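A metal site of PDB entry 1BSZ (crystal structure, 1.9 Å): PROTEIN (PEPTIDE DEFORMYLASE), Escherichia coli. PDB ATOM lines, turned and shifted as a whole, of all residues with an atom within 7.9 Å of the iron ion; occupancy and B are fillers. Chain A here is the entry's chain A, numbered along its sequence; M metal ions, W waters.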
ATOM      1  N   GLY A  45     -12.561   7.835   8.258  1.00  0.00           N
ATOM      2  CA  GLY A  45     -11.312   7.137   8.031  1.00  0.00           C
ATOM      3  C   GLY A  45     -11.245   6.732   6.575  1.00  0.00           C
ATOM      4  O   GLY A  45     -12.278   6.565   5.923  1.00  0.00           O
ATOM      5  N   LEU A  46     -10.034   6.692   6.031  1.00  0.00           N
ATOM      6  CA  LEU A  46      -9.797   6.203   4.682  1.00  0.00           C
ATOM      7  C   LEU A  46      -8.444   5.483   4.620  1.00  0.00           C
ATOM      8  O   LEU A  46      -7.486   5.902   5.267  1.00  0.00           O
ATOM      9  CB  LEU A  46      -9.816   7.373   3.682  1.00  0.00           C
ATOM     10  CG  LEU A  46     -10.070   7.003   2.221  1.00  0.00           C
ATOM     11  CD1 LEU A  46     -11.479   6.483   2.069  1.00  0.00           C
ATOM     12  CD2 LEU A  46      -9.853   8.199   1.351  1.00  0.00           C
ATOM     13  N   ALA A  47      -8.395   4.345   3.965  1.00  0.00           N
ATOM     14  CA  ALA A  47      -7.118   3.694   3.695  1.00  0.00           C
ATOM     15  C   ALA A  47      -6.767   3.928   2.222  1.00  0.00           C
ATOM     16  O   ALA A  47      -7.660   3.950   1.377  1.00  0.00           O
ATOM     17  CB  ALA A  47      -7.190   2.206   3.982  1.00  0.00           C
ATOM     18  N   GLN A  50      -8.391   1.836  -0.626  1.00  0.00           N
ATOM     19  CA  GLN A  50      -9.773   2.097  -1.015  1.00  0.00           C
ATOM     20  C   GLN A  50      -9.868   3.020  -2.223  1.00  0.00           C
ATOM     21  O   GLN A  50     -10.888   3.049  -2.920  1.00  0.00           O
ATOM     22  CB  GLN A  50     -10.534   2.749   0.125  1.00  0.00           C
ATOM     23  CG  GLN A  50     -10.844   1.806   1.230  1.00  0.00           C
ATOM     24  CD  GLN A  50     -11.563   2.501   2.343  1.00  0.00           C
ATOM     25  OE1 GLN A  50     -10.931   3.016   3.265  1.00  0.00           O
ATOM     26  NE2 GLN A  50     -12.877   2.634   2.208  1.00  0.00           N
ATOM     27  N   GLU A  88     -20.035  -0.911  12.436  1.00  0.00           N
ATOM     28  CA  GLU A  88     -19.128  -0.147  11.594  1.00  0.00           C
ATOM     29  C   GLU A  88     -19.703   0.112  10.211  1.00  0.00           C
ATOM     30  O   GLU A  88     -20.448  -0.703   9.685  1.00  0.00           O
ATOM     31  CB  GLU A  88     -17.817  -0.904  11.452  1.00  0.00           C
ATOM     32  CG  GLU A  88     -17.177  -1.214  12.772  1.00  0.00           C
ATOM     33  CD  GLU A  88     -15.787  -1.812  12.636  1.00  0.00           C
ATOM     34  OE1 GLU A  88     -15.261  -1.904  11.510  1.00  0.00           O
ATOM     35  OE2 GLU A  88     -15.232  -2.207  13.675  1.00  0.00           O
ATOM     36  N   GLY A  89     -19.295   1.220   9.614  1.00  0.00           N
ATOM     37  CA  GLY A  89     -19.554   1.436   8.202  1.00  0.00           C
ATOM     38  C   GLY A  89     -18.256   1.532   7.426  1.00  0.00           C
ATOM     39  O   GLY A  89     -17.183   1.300   7.978  1.00  0.00           O
ATOM     40  N   CYS A  90     -18.352   1.906   6.151  1.00  0.00           N
ATOM     41  CA  CYS A  90     -17.204   1.928   5.242  1.00  0.00           C
ATOM     42  C   CYS A  90     -17.686   2.534   3.935  1.00  0.00           C
ATOM     43  O   CYS A  90     -18.736   2.161   3.421  1.00  0.00           O
ATOM     44  CB  CYS A  90     -16.724   0.489   5.007  1.00  0.00           C
ATOM     45  SG  CYS A  90     -15.157   0.338   4.175  1.00  0.00           S
ATOM     46  N   LEU A  91     -16.907   3.444   3.364  1.00  0.00           N
ATOM     47  CA  LEU A  91     -17.271   4.073   2.093  1.00  0.00           C
ATOM     48  C   LEU A  91     -17.235   3.117   0.910  1.00  0.00           C
ATOM     49  O   LEU A  91     -17.794   3.411  -0.141  1.00  0.00           O
ATOM     50  CB  LEU A  91     -16.365   5.269   1.807  1.00  0.00           C
ATOM     51  CG  LEU A  91     -16.364   6.395   2.835  1.00  0.00           C
ATOM     52  CD1 LEU A  91     -15.158   7.296   2.633  1.00  0.00           C
ATOM     53  CD2 LEU A  91     -17.626   7.184   2.707  1.00  0.00           C
ATOM     54  N   SER A  92     -16.465   2.036   1.045  1.00  0.00           N
ATOM     55  CA  SER A  92     -16.400   0.972   0.024  1.00  0.00           C
ATOM     56  C   SER A  92     -17.576   0.000   0.067  1.00  0.00           C
ATOM     57  O   SER A  92     -17.721  -0.849  -0.825  1.00  0.00           O
ATOM     58  CB  SER A  92     -15.111   0.167   0.173  1.00  0.00           C
ATOM     59  OG  SER A  92     -13.991   0.970  -0.152  1.00  0.00           O
ATOM     60  N   ILE A  93     -18.350   0.045   1.155  1.00  0.00           N
ATOM     61  CA  ILE A  93     -19.525  -0.811   1.323  1.00  0.00           C
ATOM     62  C   ILE A  93     -20.736   0.080   1.639  1.00  0.00           C
ATOM     63  O   ILE A  93     -21.176   0.176   2.790  1.00  0.00           O
ATOM     64  CB  ILE A  93     -19.294  -1.872   2.423  1.00  0.00           C
ATOM     65  CG1 ILE A  93     -17.921  -2.515   2.231  1.00  0.00           C
ATOM     66  CG2 ILE A  93     -20.390  -2.934   2.364  1.00  0.00           C
ATOM     67  CD1 ILE A  93     -17.589  -3.638   3.180  1.00  0.00           C
ATOM     68  N   ARG A 102     -13.612  -6.207  17.767  1.00  0.00           N
ATOM     69  CA  ARG A 102     -12.366  -5.451  17.712  1.00  0.00           C
ATOM     70  C   ARG A 102     -11.708  -5.506  19.092  1.00  0.00           C
ATOM     71  O   ARG A 102     -12.375  -5.771  20.106  1.00  0.00           O
ATOM     72  CB  ARG A 102     -12.632  -3.989  17.348  1.00  0.00           C
ATOM     73  CG  ARG A 102     -13.246  -3.734  15.973  1.00  0.00           C
ATOM     74  CD  ARG A 102     -12.249  -4.018  14.863  1.00  0.00           C
ATOM     75  NE  ARG A 102     -12.798  -3.641  13.569  1.00  0.00           N
ATOM     76  CZ  ARG A 102     -12.362  -4.077  12.389  1.00  0.00           C
ATOM     77  NH1 ARG A 102     -11.223  -4.768  12.286  1.00  0.00           N
ATOM     78  NH2 ARG A 102     -13.015  -3.728  11.290  1.00  0.00           N
ATOM     79  N   CYS A 129     -11.469   2.396  14.843  1.00  0.00           N
ATOM     80  CA  CYS A 129     -11.214   3.037  13.561  1.00  0.00           C
ATOM     81  C   CYS A 129      -9.834   2.699  13.008  1.00  0.00           C
ATOM     82  O   CYS A 129      -9.695   2.471  11.813  1.00  0.00           O
ATOM     83  CB  CYS A 129     -11.330   4.541  13.762  1.00  0.00           C
ATOM     84  SG  CYS A 129     -11.159   5.436  12.261  1.00  0.00           S
ATOM     85  N   HIS A 132      -9.916  -1.089  11.893  1.00  0.00           N
ATOM     86  CA  HIS A 132     -10.677  -1.173  10.660  1.00  0.00           C
ATOM     87  C   HIS A 132      -9.818  -0.665   9.483  1.00  0.00           C
ATOM     88  O   HIS A 132      -9.821  -1.241   8.393  1.00  0.00           O
ATOM     89  CB  HIS A 132     -11.940  -0.319  10.834  1.00  0.00           C
ATOM     90  CG  HIS A 132     -12.730  -0.114   9.587  1.00  0.00           C
ATOM     91  ND1 HIS A 132     -14.053  -0.487   9.477  1.00  0.00           N
ATOM     92  CD2 HIS A 132     -12.399   0.463   8.407  1.00  0.00           C
ATOM     93  CE1 HIS A 132     -14.500  -0.149   8.276  1.00  0.00           C
ATOM     94  NE2 HIS A 132     -13.522   0.428   7.614  1.00  0.00           N
ATOM     95  N   GLU A 133      -9.087   0.421   9.682  1.00  0.00           N
ATOM     96  CA  GLU A 133      -8.288   0.988   8.603  1.00  0.00           C
ATOM     97  C   GLU A 133      -7.042   0.154   8.342  1.00  0.00           C
ATOM     98  O   GLU A 133      -6.697  -0.098   7.201  1.00  0.00           O
ATOM     99  CB  GLU A 133      -7.876   2.437   8.919  1.00  0.00           C
ATOM    100  CG  GLU A 133      -9.029   3.431   8.879  1.00  0.00           C
ATOM    101  CD  GLU A 133      -9.915   3.288   7.653  1.00  0.00           C
ATOM    102  OE1 GLU A 133      -9.387   3.097   6.537  1.00  0.00           O
ATOM    103  OE2 GLU A 133     -11.147   3.449   7.812  1.00  0.00           O
ATOM    104  N   ASP A 135      -6.853  -2.947   8.662  1.00  0.00           N
ATOM    105  CA  ASP A 135      -7.343  -4.133   7.945  1.00  0.00           C
ATOM    106  C   ASP A 135      -7.305  -3.898   6.443  1.00  0.00           C
ATOM    107  O   ASP A 135      -6.980  -4.802   5.689  1.00  0.00           O
ATOM    108  CB  ASP A 135      -8.798  -4.504   8.338  1.00  0.00           C
ATOM    109  CG  ASP A 135      -8.876  -5.477   9.523  1.00  0.00           C
ATOM    110  OD1 ASP A 135      -7.824  -5.922  10.018  1.00  0.00           O
ATOM    111  OD2 ASP A 135     -10.000  -5.774   9.978  1.00  0.00           O
ATOM    112  N   HIS A 136      -7.762  -2.732   5.999  1.00  0.00           N
ATOM    113  CA  HIS A 136      -7.838  -2.423   4.579  1.00  0.00           C
ATOM    114  C   HIS A 136      -6.523  -2.689   3.871  1.00  0.00           C
ATOM    115  O   HIS A 136      -6.508  -3.138   2.724  1.00  0.00           O
ATOM    116  CB  HIS A 136      -8.212  -0.967   4.345  1.00  0.00           C
ATOM    117  CG  HIS A 136      -9.682  -0.712   4.426  1.00  0.00           C
ATOM    118  ND1 HIS A 136     -10.593  -1.331   3.594  1.00  0.00           N
ATOM    119  CD2 HIS A 136     -10.398   0.111   5.226  1.00  0.00           C
ATOM    120  CE1 HIS A 136     -11.803  -0.878   3.858  1.00  0.00           C
ATOM    121  NE2 HIS A 136     -11.714   0.000   4.847  1.00  0.00           N
ATOM    122  N   LYS A 140      -8.403  -6.795   4.038  1.00  0.00           N
ATOM    123  CA  LYS A 140      -9.563  -7.197   4.853  1.00  0.00           C
ATOM    124  C   LYS A 140     -10.657  -6.132   4.890  1.00  0.00           C
ATOM    125  O   LYS A 140     -10.371  -4.957   5.162  1.00  0.00           O
ATOM    126  CB  LYS A 140      -9.141  -7.458   6.290  1.00  0.00           C
ATOM    127  CG  LYS A 140      -8.488  -8.788   6.550  1.00  0.00           C
ATOM    128  CD  LYS A 140      -9.247  -9.539   7.644  1.00  0.00           C
ATOM    129  CE  LYS A 140      -8.333  -9.995   8.769  1.00  0.00           C
ATOM    130  NZ  LYS A 140      -9.124 -10.477   9.940  1.00  0.00           N
ATOM    131  N   LEU A 141     -11.912  -6.576   4.838  1.00  0.00           N
ATOM    132  CA  LEU A 141     -13.091  -5.710   4.923  1.00  0.00           C
ATOM    133  C   LEU A 141     -13.917  -6.139   6.152  1.00  0.00           C
ATOM    134  O   LEU A 141     -13.779  -7.265   6.603  1.00  0.00           O
ATOM    135  CB  LEU A 141     -13.931  -5.871   3.659  1.00  0.00           C
ATOM    136  CG  LEU A 141     -13.297  -5.426   2.337  1.00  0.00           C
ATOM    137  CD1 LEU A 141     -14.130  -5.924   1.162  1.00  0.00           C
ATOM    138  CD2 LEU A 141     -13.180  -3.909   2.308  1.00  0.00           C
ATOM    139  N   PHE A 142     -14.788  -5.281   6.685  1.00  0.00           N
ATOM    140  CA  PHE A 142     -15.440  -5.635   7.956  1.00  0.00           C
ATOM    141  C   PHE A 142     -16.446  -6.772   7.788  1.00  0.00           C
ATOM    142  O   PHE A 142     -16.684  -7.543   8.709  1.00  0.00           O
ATOM    143  CB  PHE A 142     -16.054  -4.404   8.689  1.00  0.00           C
ATOM    144  CG  PHE A 142     -17.358  -3.920   8.122  1.00  0.00           C
ATOM    145  CD1 PHE A 142     -18.512  -4.672   8.234  1.00  0.00           C
ATOM    146  CD2 PHE A 142     -17.418  -2.732   7.406  1.00  0.00           C
ATOM    147  CE1 PHE A 142     -19.704  -4.266   7.627  1.00  0.00           C
ATOM    148  CE2 PHE A 142     -18.610  -2.317   6.802  1.00  0.00           C
ATOM    149  CZ  PHE A 142     -19.752  -3.081   6.919  1.00  0.00           C
HETATM  150 FE    FE M   1     -13.451   0.998   5.572  1.00  0.00          FE
HETATM  151  O   HOH W   1     -12.459   2.952   5.642  1.00  0.00           O
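A ring nitrogen (NE2) of His 136 sits close to the side-chain amide oxygen (OE1) of Gln 50 (3.5 Å). A ring nitrogen (ND1) of His 132 is in hydrogen-bond range of the side-chain carboxylate of Glu 88 (2.8 Å). The side-chain hydroxyl of Ser 92 sits at hydrogen-bond distance from the side-chain amide nitrogen of Gln 50 (3.1 Å). The side-chain amide oxygen of Gln 50 is in hydrogen-bond range of the backbone NH of Ala 47 (2.9 Å). The side-chain sulfur (SG) of Cys 90 sits close to the side-chain amide nitrogen (NE2) of Gln 50. SG of Cys 90 lies close to N of Ser 92 (3.8 Å).
Gln 50 touches the iron ion.
The iron ion is bound by a ring nitrogen (NE2) of His 132 (2.1 Å), a ring nitrogen (NE2) of His 136 (2.1 Å), water W1 (2.2 Å) and the side-chain sulfur (SG) of Cys 90 (2.3 Å).
Water W1 bridges OE2 of Glu 133 (2.6 Å) and OE1 of Gln 50 (2.8 Å).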
